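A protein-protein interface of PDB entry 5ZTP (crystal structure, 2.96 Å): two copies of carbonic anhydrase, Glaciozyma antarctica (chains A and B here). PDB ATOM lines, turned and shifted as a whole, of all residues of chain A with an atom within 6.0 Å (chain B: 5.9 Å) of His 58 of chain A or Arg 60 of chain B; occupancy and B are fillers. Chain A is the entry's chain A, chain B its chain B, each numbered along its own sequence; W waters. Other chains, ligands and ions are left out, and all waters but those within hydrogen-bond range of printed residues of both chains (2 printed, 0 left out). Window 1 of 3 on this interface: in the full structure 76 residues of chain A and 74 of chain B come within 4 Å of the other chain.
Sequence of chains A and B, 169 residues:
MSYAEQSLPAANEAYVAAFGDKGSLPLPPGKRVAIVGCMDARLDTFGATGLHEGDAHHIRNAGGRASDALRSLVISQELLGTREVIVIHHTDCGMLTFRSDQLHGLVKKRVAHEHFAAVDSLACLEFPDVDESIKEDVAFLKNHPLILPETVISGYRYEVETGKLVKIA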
ATOM      1  N   VAL A  33      33.005  -6.344  -0.470  1.00  0.00           N
ATOM      2  CA  VAL A  33      31.687  -6.515  -1.055  1.00  0.00           C
ATOM      3  C   VAL A  33      30.827  -5.320  -0.714  1.00  0.00           C
ATOM      4  O   VAL A  33      30.846  -4.835   0.436  1.00  0.00           O
ATOM      5  CB  VAL A  33      30.949  -7.745  -0.489  1.00  0.00           C
ATOM      6  CG1 VAL A  33      29.632  -7.965  -1.226  1.00  0.00           C
ATOM      7  CG2 VAL A  33      31.796  -9.001  -0.585  1.00  0.00           C
ATOM      8  N   ALA A  34      30.053  -4.881  -1.707  1.00  0.00           N
ATOM      9  CA  ALA A  34      29.052  -3.881  -1.487  1.00  0.00           C
ATOM     10  C   ALA A  34      27.724  -4.505  -1.811  1.00  0.00           C
ATOM     11  O   ALA A  34      27.512  -4.965  -2.927  1.00  0.00           O
ATOM     12  CB  ALA A  34      29.305  -2.696  -2.371  1.00  0.00           C
ATOM     13  N   ILE A  35      26.839  -4.558  -0.828  1.00  0.00           N
ATOM     14  CA  ILE A  35      25.471  -5.040  -1.059  1.00  0.00           C
ATOM     15  C   ILE A  35      24.629  -3.863  -1.518  1.00  0.00           C
ATOM     16  O   ILE A  35      24.688  -2.795  -0.914  1.00  0.00           O
ATOM     17  CB  ILE A  35      24.815  -5.637   0.224  1.00  0.00           C
ATOM     18  CG1 ILE A  35      25.621  -6.832   0.783  1.00  0.00           C
ATOM     19  CG2 ILE A  35      23.370  -6.029  -0.035  1.00  0.00           C
ATOM     20  CD1 ILE A  35      26.141  -7.829  -0.239  1.00  0.00           C
ATOM     21  N   THR A  45      20.201  -7.732   5.188  1.00  0.00           N
ATOM     22  CA  THR A  45      21.327  -7.978   4.317  1.00  0.00           C
ATOM     23  C   THR A  45      22.562  -8.521   5.037  1.00  0.00           C
ATOM     24  O   THR A  45      23.570  -8.824   4.397  1.00  0.00           O
ATOM     25  CB  THR A  45      21.681  -6.677   3.593  1.00  0.00           C
ATOM     26  OG1 THR A  45      21.692  -5.593   4.535  1.00  0.00           O
ATOM     27  CG2 THR A  45      20.641  -6.396   2.530  1.00  0.00           C
ATOM     28  N   PHE A  46      22.499  -8.618   6.366  1.00  0.00           N
ATOM     29  CA  PHE A  46      23.497  -9.380   7.115  1.00  0.00           C
ATOM     30  C   PHE A  46      23.152 -10.868   7.065  1.00  0.00           C
ATOM     31  O   PHE A  46      23.755 -11.651   6.307  1.00  0.00           O
ATOM     32  CB  PHE A  46      23.578  -8.900   8.561  1.00  0.00           C
ATOM     33  CG  PHE A  46      24.513  -7.754   8.769  1.00  0.00           C
ATOM     34  CD1 PHE A  46      24.268  -6.524   8.181  1.00  0.00           C
ATOM     35  CD2 PHE A  46      25.645  -7.903   9.568  1.00  0.00           C
ATOM     36  CE1 PHE A  46      25.137  -5.464   8.396  1.00  0.00           C
ATOM     37  CE2 PHE A  46      26.511  -6.847   9.783  1.00  0.00           C
ATOM     38  CZ  PHE A  46      26.254  -5.622   9.210  1.00  0.00           C
ATOM     39  N   THR A  49      22.360 -13.186   4.083  1.00  0.00           N
ATOM     40  CA  THR A  49      23.528 -13.540   3.300  1.00  0.00           C
ATOM     41  C   THR A  49      24.862 -13.798   4.037  1.00  0.00           C
ATOM     42  O   THR A  49      25.922 -13.697   3.449  1.00  0.00           O
ATOM     43  CB  THR A  49      23.708 -12.500   2.212  1.00  0.00           C
ATOM     44  OG1 THR A  49      24.885 -12.835   1.485  1.00  0.00           O
ATOM     45  CG2 THR A  49      23.806 -11.106   2.798  1.00  0.00           C
ATOM     46  N   LEU A  51      26.716 -12.415   6.066  1.00  0.00           N
ATOM     47  CA  LEU A  51      27.644 -11.336   6.230  1.00  0.00           C
ATOM     48  C   LEU A  51      27.495 -10.825   7.647  1.00  0.00           C
ATOM     49  O   LEU A  51      26.371 -10.637   8.124  1.00  0.00           O
ATOM     50  CB  LEU A  51      27.364 -10.244   5.208  1.00  0.00           C
ATOM     51  CG  LEU A  51      27.749 -10.605   3.770  1.00  0.00           C
ATOM     52  CD1 LEU A  51      27.166  -9.613   2.791  1.00  0.00           C
ATOM     53  CD2 LEU A  51      29.249 -10.627   3.588  1.00  0.00           C
ATOM     54  N   HIS A  52      28.645 -10.652   8.316  1.00  0.00           N
ATOM     55  CA  HIS A  52      28.719 -10.171   9.702  1.00  0.00           C
ATOM     56  C   HIS A  52      29.475  -8.871   9.751  1.00  0.00           C
ATOM     57  O   HIS A  52      30.033  -8.417   8.759  1.00  0.00           O
ATOM     58  CB  HIS A  52      29.413 -11.207  10.600  1.00  0.00           C
ATOM     59  CG  HIS A  52      28.752 -12.545  10.563  1.00  0.00           C
ATOM     60  ND1 HIS A  52      27.567 -12.802  11.223  1.00  0.00           N
ATOM     61  CD2 HIS A  52      29.068 -13.679   9.891  1.00  0.00           C
ATOM     62  CE1 HIS A  52      27.193 -14.042  10.975  1.00  0.00           C
ATOM     63  NE2 HIS A  52      28.082 -14.593  10.167  1.00  0.00           N
ATOM     64  N   ASP A  55      32.273  -7.159   7.225  1.00  0.00           N
ATOM     65  CA  ASP A  55      32.489  -7.920   5.988  1.00  0.00           C
ATOM     66  C   ASP A  55      32.201  -7.118   4.716  1.00  0.00           C
ATOM     67  O   ASP A  55      32.972  -7.178   3.756  1.00  0.00           O
ATOM     68  CB  ASP A  55      31.653  -9.216   6.001  1.00  0.00           C
ATOM     69  CG  ASP A  55      32.122 -10.212   7.058  1.00  0.00           C
ATOM     70  OD1 ASP A  55      33.141  -9.924   7.742  1.00  0.00           O
ATOM     71  OD2 ASP A  55      31.451 -11.267   7.214  1.00  0.00           O
ATOM     72  N   ALA A  56      31.091  -6.383   4.700  1.00  0.00           N
ATOM     73  CA  ALA A  56      30.608  -5.777   3.461  1.00  0.00           C
ATOM     74  C   ALA A  56      29.922  -4.461   3.700  1.00  0.00           C
ATOM     75  O   ALA A  56      29.436  -4.197   4.782  1.00  0.00           O
ATOM     76  CB  ALA A  56      29.634  -6.714   2.795  1.00  0.00           C
ATOM     77  N   HIS A  57      29.865  -3.649   2.658  1.00  0.00           N
ATOM     78  CA  HIS A  57      29.098  -2.437   2.717  1.00  0.00           C
ATOM     79  C   HIS A  57      27.649  -2.727   2.417  1.00  0.00           C
ATOM     80  O   HIS A  57      27.342  -3.512   1.517  1.00  0.00           O
ATOM     81  CB  HIS A  57      29.613  -1.413   1.728  1.00  0.00           C
ATOM     82  CG  HIS A  57      30.758  -0.618   2.252  1.00  0.00           C
ATOM     83  ND1 HIS A  57      31.827  -0.245   1.464  1.00  0.00           N
ATOM     84  CD2 HIS A  57      31.011  -0.142   3.493  1.00  0.00           C
ATOM     85  CE1 HIS A  57      32.691   0.428   2.201  1.00  0.00           C
ATOM     86  NE2 HIS A  57      32.218   0.505   3.435  1.00  0.00           N
ATOM     87  N   HIS A  58      26.768  -2.062   3.166  1.00  0.00           N
ATOM     88  CA  HIS A  58      25.343  -2.216   3.004  1.00  0.00           C
ATOM     89  C   HIS A  58      24.675  -0.938   2.533  1.00  0.00           C
ATOM     90  O   HIS A  58      24.367  -0.057   3.328  1.00  0.00           O
ATOM     91  CB  HIS A  58      24.767  -2.695   4.310  1.00  0.00           C
ATOM     92  CG  HIS A  58      25.349  -3.993   4.746  1.00  0.00           C
ATOM     93  ND1 HIS A  58      24.789  -5.208   4.416  1.00  0.00           N
ATOM     94  CD2 HIS A  58      26.471  -4.272   5.448  1.00  0.00           C
ATOM     95  CE1 HIS A  58      25.526  -6.182   4.919  1.00  0.00           C
ATOM     96  NE2 HIS A  58      26.558  -5.642   5.546  1.00  0.00           N
ATOM     97  N   ILE A  59      24.457  -0.863   1.223  1.00  0.00           N
ATOM     98  CA  ILE A  59      23.795   0.268   0.590  1.00  0.00           C
ATOM     99  C   ILE A  59      22.314  -0.075   0.286  1.00  0.00           C
ATOM    100  O   ILE A  59      21.997  -0.997  -0.467  1.00  0.00           O
ATOM    101  CB  ILE A  59      24.549   0.679  -0.697  1.00  0.00           C
ATOM    102  CG1 ILE A  59      26.061   0.853  -0.410  1.00  0.00           C
ATOM    103  CG2 ILE A  59      23.948   1.951  -1.288  1.00  0.00           C
ATOM    104  CD1 ILE A  59      26.974   0.761  -1.625  1.00  0.00           C
ATOM    105  N   ARG A  60      21.401   0.669   0.881  1.00  0.00           N
ATOM    106  CA  ARG A  60      19.992   0.335   0.788  1.00  0.00           C
ATOM    107  C   ARG A  60      19.133   1.587   0.554  1.00  0.00           C
ATOM    108  O   ARG A  60      19.329   2.638   1.192  1.00  0.00           O
ATOM    109  CB  ARG A  60      19.529  -0.425   2.039  1.00  0.00           C
ATOM    110  CG  ARG A  60      20.145  -1.817   2.255  1.00  0.00           C
ATOM    111  CD  ARG A  60      20.000  -2.301   3.719  1.00  0.00           C
ATOM    112  NE  ARG A  60      19.047  -3.237   4.368  1.00  0.00           N
ATOM    113  CZ  ARG A  60      17.870  -3.639   3.960  1.00  0.00           C
ATOM    114  NH1 ARG A  60      17.369  -3.230   2.837  1.00  0.00           N
ATOM    115  NH2 ARG A  60      17.182  -4.475   4.709  1.00  0.00           N
ATOM    116  N   ASN A  61      18.211   1.471  -0.406  1.00  0.00           N
ATOM    117  CA  ASN A  61      17.324   2.545  -0.766  1.00  0.00           C
ATOM    118  C   ASN A  61      16.039   1.949  -1.287  1.00  0.00           C
ATOM    119  O   ASN A  61      15.975   0.755  -1.537  1.00  0.00           O
ATOM    120  CB  ASN A  61      17.974   3.431  -1.812  1.00  0.00           C
ATOM    121  CG  ASN A  61      18.176   2.729  -3.169  1.00  0.00           C
ATOM    122  OD1 ASN A  61      17.206   2.413  -3.868  1.00  0.00           O
ATOM    123  ND2 ASN A  61      19.437   2.563  -3.579  1.00  0.00           N
ATOM    124  N   SER A  72      27.329   6.013  -3.410  1.00  0.00           N
ATOM    125  CA  SER A  72      27.824   5.226  -2.295  1.00  0.00           C
ATOM    126  C   SER A  72      28.820   4.204  -2.808  1.00  0.00           C
ATOM    127  O   SER A  72      29.806   3.895  -2.145  1.00  0.00           O
ATOM    128  CB  SER A  72      26.669   4.516  -1.577  1.00  0.00           C
ATOM    129  OG  SER A  72      25.869   5.414  -0.828  1.00  0.00           O
ATOM    130  N   ILE B  35      15.128   3.588   9.389  1.00  0.00           N
ATOM    131  CA  ILE B  35      16.504   3.802   9.845  1.00  0.00           C
ATOM    132  C   ILE B  35      17.268   4.485   8.724  1.00  0.00           C
ATOM    133  O   ILE B  35      17.171   4.071   7.573  1.00  0.00           O
ATOM    134  CB  ILE B  35      17.235   2.477  10.199  1.00  0.00           C
ATOM    135  CG1 ILE B  35      16.506   1.692  11.312  1.00  0.00           C
ATOM    136  CG2 ILE B  35      18.687   2.738  10.567  1.00  0.00           C
ATOM    137  CD1 ILE B  35      15.992   2.513  12.479  1.00  0.00           C
ATOM    138  N   VAL B  36      18.019   5.528   9.049  1.00  0.00           N
ATOM    139  CA  VAL B  36      18.901   6.120   8.069  1.00  0.00           C
ATOM    140  C   VAL B  36      20.317   6.017   8.580  1.00  0.00           C
ATOM    141  O   VAL B  36      20.720   6.785   9.447  1.00  0.00           O
ATOM    142  CB  VAL B  36      18.554   7.589   7.780  1.00  0.00           C
ATOM    143  CG1 VAL B  36      19.541   8.157   6.757  1.00  0.00           C
ATOM    144  CG2 VAL B  36      17.110   7.695   7.299  1.00  0.00           C
ATOM    145  N   GLY B  37      21.071   5.070   8.040  1.00  0.00           N
ATOM    146  CA  GLY B  37      22.381   4.758   8.590  1.00  0.00           C
ATOM    147  C   GLY B  37      23.472   4.765   7.545  1.00  0.00           C
ATOM    148  O   GLY B  37      23.241   4.528   6.367  1.00  0.00           O
ATOM    149  N   CYS B  38      24.686   5.041   7.977  1.00  0.00           N
ATOM    150  CA  CYS B  38      25.774   4.889   7.077  1.00  0.00           C
ATOM    151  C   CYS B  38      25.905   3.450   6.606  1.00  0.00           C
ATOM    152  O   CYS B  38      25.459   2.543   7.282  1.00  0.00           O
ATOM    153  CB  CYS B  38      27.057   5.283   7.730  1.00  0.00           C
ATOM    154  SG  CYS B  38      28.395   5.103   6.506  1.00  0.00           S
ATOM    155  N   MET B  39      26.552   3.263   5.461  1.00  0.00           N
ATOM    156  CA  MET B  39      26.735   1.944   4.863  1.00  0.00           C
ATOM    157  C   MET B  39      27.886   1.139   5.479  1.00  0.00           C
ATOM    158  O   MET B  39      28.198   0.066   4.983  1.00  0.00           O
ATOM    159  CB  MET B  39      27.025   2.092   3.355  1.00  0.00           C
ATOM    160  CG  MET B  39      28.408   2.694   3.027  1.00  0.00           C
ATOM    161  SD  MET B  39      28.875   2.750   1.293  1.00  0.00           S
ATOM    162  CE  MET B  39      30.380   3.709   1.332  1.00  0.00           C
ATOM    163  N   ASP B  40      28.531   1.676   6.516  1.00  0.00           N
ATOM    164  CA  ASP B  40      29.751   1.093   7.108  1.00  0.00           C
ATOM    165  C   ASP B  40      29.537  -0.357   7.475  1.00  0.00           C
ATOM    166  O   ASP B  40      28.536  -0.700   8.107  1.00  0.00           O
ATOM    167  CB  ASP B  40      30.168   1.863   8.369  1.00  0.00           C
ATOM    168  CG  ASP B  40      31.464   1.358   8.976  1.00  0.00           C
ATOM    169  OD1 ASP B  40      32.559   1.677   8.462  1.00  0.00           O
ATOM    170  OD2 ASP B  40      31.378   0.658  10.003  1.00  0.00           O
ATOM    171  N   ALA B  41      30.500  -1.194   7.093  1.00  0.00           N
ATOM    172  CA  ALA B  41      30.348  -2.643   7.155  1.00  0.00           C
ATOM    173  C   ALA B  41      30.161  -3.149   8.559  1.00  0.00           C
ATOM    174  O   ALA B  41      29.597  -4.222   8.740  1.00  0.00           O
ATOM    175  CB  ALA B  41      31.557  -3.309   6.553  1.00  0.00           C
ATOM    176  N   ARG B  42      30.653  -2.376   9.534  1.00  0.00           N
ATOM    177  CA  ARG B  42      30.647  -2.766  10.928  1.00  0.00           C
ATOM    178  C   ARG B  42      29.341  -2.498  11.641  1.00  0.00           C
ATOM    179  O   ARG B  42      29.239  -2.784  12.823  1.00  0.00           O
ATOM    180  CB  ARG B  42      31.729  -2.018  11.653  1.00  0.00           C
ATOM    181  CG  ARG B  42      33.117  -2.356  11.156  1.00  0.00           C
ATOM    182  CD  ARG B  42      34.128  -1.325  11.635  1.00  0.00           C
ATOM    183  NE  ARG B  42      33.907  -0.027  11.019  1.00  0.00           N
ATOM    184  CZ  ARG B  42      34.713   1.024  11.153  1.00  0.00           C
ATOM    185  NH1 ARG B  42      35.811   0.936  11.898  1.00  0.00           N
ATOM    186  NH2 ARG B  42      34.429   2.169  10.524  1.00  0.00           N
ATOM    187  N   LEU B  43      28.354  -1.943  10.936  1.00  0.00           N
ATOM    188  CA  LEU B  43      27.063  -1.587  11.529  1.00  0.00           C
ATOM    189  C   LEU B  43      25.968  -2.460  10.953  1.00  0.00           C
ATOM    190  O   LEU B  43      25.791  -2.548   9.751  1.00  0.00           O
ATOM    191  CB  LEU B  43      26.730  -0.122  11.263  1.00  0.00           C
ATOM    192  CG  LEU B  43      25.306   0.395  11.550  1.00  0.00           C
ATOM    193  CD1 LEU B  43      24.969   0.435  13.036  1.00  0.00           C
ATOM    194  CD2 LEU B  43      25.151   1.787  10.948  1.00  0.00           C
ATOM    195  N   ASP B  44      25.248  -3.126  11.836  1.00  0.00           N
ATOM    196  CA  ASP B  44      24.098  -3.867  11.448  1.00  0.00           C
ATOM    197  C   ASP B  44      22.954  -3.172  12.092  1.00  0.00           C
ATOM    198  O   ASP B  44      22.782  -3.255  13.292  1.00  0.00           O
ATOM    199  CB  ASP B  44      24.114  -5.285  11.946  1.00  0.00           C
ATOM    200  CG  ASP B  44      22.764  -5.935  11.791  1.00  0.00           C
ATOM    201  OD1 ASP B  44      22.116  -5.758  10.728  1.00  0.00           O
ATOM    202  OD2 ASP B  44      22.321  -6.588  12.745  1.00  0.00           O
ATOM    203  N   THR B  45      22.154  -2.524  11.263  1.00  0.00           N
ATOM    204  CA  THR B  45      21.000  -1.763  11.691  1.00  0.00           C
ATOM    205  C   THR B  45      19.825  -2.621  12.157  1.00  0.00           C
ATOM    206  O   THR B  45      18.808  -2.090  12.606  1.00  0.00           O
ATOM    207  CB  THR B  45      20.557  -0.857  10.539  1.00  0.00           C
ATOM    208  OG1 THR B  45      20.537  -1.618   9.321  1.00  0.00           O
ATOM    209  CG2 THR B  45      21.541   0.294  10.383  1.00  0.00           C
ATOM    210  N   HIS B  58      15.221   0.060   6.280  1.00  0.00           N
ATOM    211  CA  HIS B  58      16.652   0.271   6.392  1.00  0.00           C
ATOM    212  C   HIS B  58      17.221   0.975   5.176  1.00  0.00           C
ATOM    213  O   HIS B  58      17.492   0.351   4.154  1.00  0.00           O
ATOM    214  CB  HIS B  58      17.316  -1.061   6.630  1.00  0.00           C
ATOM    215  CG  HIS B  58      16.813  -1.737   7.859  1.00  0.00           C
ATOM    216  ND1 HIS B  58      17.415  -1.581   9.088  1.00  0.00           N
ATOM    217  CD2 HIS B  58      15.726  -2.524   8.066  1.00  0.00           C
ATOM    218  CE1 HIS B  58      16.741  -2.271   9.996  1.00  0.00           C
ATOM    219  NE2 HIS B  58      15.709  -2.850   9.404  1.00  0.00           N
ATOM    220  N   ILE B  59      17.390   2.288   5.307  1.00  0.00           N
ATOM    221  CA  ILE B  59      17.969   3.138   4.264  1.00  0.00           C
ATOM    222  C   ILE B  59      19.450   3.459   4.588  1.00  0.00           C
ATOM    223  O   ILE B  59      19.788   4.062   5.608  1.00  0.00           O
ATOM    224  CB  ILE B  59      17.145   4.441   4.105  1.00  0.00           C
ATOM    225  CG1 ILE B  59      15.641   4.116   3.948  1.00  0.00           C
ATOM    226  CG2 ILE B  59      17.658   5.257   2.923  1.00  0.00           C
ATOM    227  CD1 ILE B  59      14.686   5.254   4.273  1.00  0.00           C
ATOM    228  N   ARG B  60      20.336   3.042   3.708  1.00  0.00           N
ATOM    229  CA  ARG B  60      21.746   3.160   3.975  1.00  0.00           C
ATOM    230  C   ARG B  60      22.539   3.658   2.756  1.00  0.00           C
ATOM    231  O   ARG B  60      22.333   3.200   1.613  1.00  0.00           O
ATOM    232  CB  ARG B  60      22.291   1.831   4.474  1.00  0.00           C
ATOM    233  CG  ARG B  60      21.716   1.371   5.829  1.00  0.00           C
ATOM    234  CD  ARG B  60      22.154  -0.054   6.146  1.00  0.00           C
ATOM    235  NE  ARG B  60      23.491   0.081   6.744  1.00  0.00           N
ATOM    236  CZ  ARG B  60      24.157  -0.826   7.425  1.00  0.00           C
ATOM    237  NH1 ARG B  60      23.678  -2.040   7.632  1.00  0.00           N
ATOM    238  NH2 ARG B  60      25.329  -0.497   7.901  1.00  0.00           N
ATOM    239  N   ASN B  61      23.425   4.625   3.012  1.00  0.00           N
ATOM    240  CA  ASN B  61      24.272   5.193   1.987  1.00  0.00           C
ATOM    241  C   ASN B  61      25.574   5.651   2.621  1.00  0.00           C
ATOM    242  O   ASN B  61      25.683   5.703   3.830  1.00  0.00           O
ATOM    243  CB  ASN B  61      23.551   6.344   1.298  1.00  0.00           C
ATOM    244  CG  ASN B  61      23.315   7.548   2.215  1.00  0.00           C
ATOM    245  OD1 ASN B  61      24.273   8.225   2.624  1.00  0.00           O
ATOM    246  ND2 ASN B  61      22.041   7.850   2.503  1.00  0.00           N
ATOM    247  N   ALA B  62      26.543   5.985   1.774  1.00  0.00           N
ATOM    248  CA  ALA B  62      27.848   6.484   2.219  1.00  0.00           C
ATOM    249  C   ALA B  62      27.616   7.648   3.149  1.00  0.00           C
ATOM    250  O   ALA B  62      27.032   8.634   2.728  1.00  0.00           O
ATOM    251  CB  ALA B  62      28.692   6.925   1.035  1.00  0.00           C
ATOM    252  N   GLY B  64      25.581   7.827   5.655  1.00  0.00           N
ATOM    253  CA  GLY B  64      24.300   7.791   6.314  1.00  0.00           C
ATOM    254  C   GLY B  64      23.576   9.118   6.174  1.00  0.00           C
ATOM    255  O   GLY B  64      22.883   9.566   7.104  1.00  0.00           O
HETATM  256  O   HOH W   1      28.941  -6.426   7.028  1.00  0.00           O
HETATM  257  O   HOH W   2      32.956   0.301   6.134  1.00  0.00           O
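The backbone NH (N) of His 58 of chain A is in hydrogen-bond range of the backbone carbonyl oxygen (O) of Met 39 of chain B. N of Arg 60 of chain B sits at hydrogen-bond distance from O of Arg 60 of chain A. The side-chain hydroxyl (OG) of Ser 72 of chain A is in hydrogen-bond range of the backbone NH (N) of Ala 62 of chain B (2.7 Å). The backbone carbonyl oxygen (O) of Ser 72 of chain A sits close to the side-chain sulfur (SD) of Met 39 of chain B (3.7 Å).
ND1 of His 58 of chain B is in hydrogen-bond range of OG1 of Thr 45 of chain B (3.1 Å). The backbone carbonyl oxygen (O) of Cys 38 of chain B lies within hydrogen-bond range of the guanidinium group (NH2) of Arg 60 of chain B (3.1 Å). The guanidinium group of Arg 60 of chain B is in hydrogen-bond range of the backbone carbonyl oxygen of Leu 43 of chain B (2.8 Å). The backbone NH (N) of His 57 of chain A lies within hydrogen-bond range of the backbone carbonyl oxygen (O) of Val 33 of chain A (2.7 Å). The backbone NH of His 52 of chain A lies within hydrogen-bond range of the side-chain carboxylate of Asp 55 of chain A (3.1 Å). The backbone carbonyl oxygen (O) of Phe 46 of chain A is in hydrogen-bond range of the backbone NH (N) of Leu 51 of chain A, at 3.1 Å.
Among the printed residues, merely in contact across the chains: Ala 56 of chain A with Ala 41 of chain B (2.9 Å), His 58 of chain A with Arg 60 of chain B (3.0 Å), Arg 60 of chain A with His 58 of chain B (3.0 Å), Phe 46 of chain A with Leu 43 of chain B (3.2 Å), His 57 of chain A with Met 39 of chain B (3.2 Å), Ser 72 of chain A with Asn 61 of chain B (3.2 Å), Arg 60 of chain A with Ile 59 of chain B (3.4 Å), Phe 46 of chain A with Asp 44 of chain B (3.4 Å), Ile 59 of chain A with Arg 60 of chain B (3.4 Å), Phe 46 of chain A with Ala 41 of chain B (3.7 Å), His 57 of chain A with Ala 41 of chain B (3.8 Å), Ile 59 of chain A with Met 39 of chain B (3.8 Å), Phe 46 of chain A with Arg 60 of chain B (3.8 Å) and Asp 55 of chain A with Ala 41 of chain B (3.97 Å).
Of the printed residues of chain B, Ala 56 of chain A touches Ala 41. Of chain B, only Met 39 (3.1 Å) and Arg 60 (3.0 Å) come within 4 Å of His 58 of chain A. Of the printed residues of chain B, Arg 60 of chain A touches His 58 (3.0 Å), Ile 59 (3.4 Å) and Arg 60 (2.7 Å). Of the printed residues of chain A, His 58 of chain B touches Arg 60. Of the printed residues of chain A, Ile 59 of chain B touches Arg 60 (3.4 Å). Printed residues of chain A within 4 Å of Arg 60 of chain B: Phe 46, His 58, Ile 59 and Arg 60. The nearest printed residue of chain B that does not touch Arg 60 of chain A is Asn 61 of chain B (4.9 Å).
Of the 16 printed residues of chain A, 8 touch a printed residue of chain B. Among the printed residues, no Asp or Glu carboxylate lies within 4 Å of a Lys or Arg side-chain nitrogen of the other chain.
His 58 of chain A touches Arg 60 of chain B, and with the chains exchanged Arg 60 of chain A touches His 58 of chain B. Ile 59 of chain A touches Arg 60 of chain B, and with the chains exchanged Arg 60 of chain A touches Ile 59 of chain B. Arg 60 of chain A touches its own counterpart, Arg 60 of chain B. Positions printed for both chains: 35, 45, 58, 59, 60 and 61. Of the 18 pairs that touch across the chains among the printed residues, 5 have their exchanged pair printed and touching as well.
Water W2 lies within hydrogen-bond range of OD1 of Asp 40 of chain B (2.7 Å), NE2 of His 57 of chain A (2.8 Å) and N of Ala 41 of chain B (3.0 Å). Water W1 lies within hydrogen-bond range of O of His 52 of chain A (2.9 Å), O of Ala 41 of chain B (2.9 Å), NE2 of His 58 of chain A (2.9 Å), N of Ala 56 of chain A (3.2 Å) and N of Asp 55 of chain A (3.4 Å).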
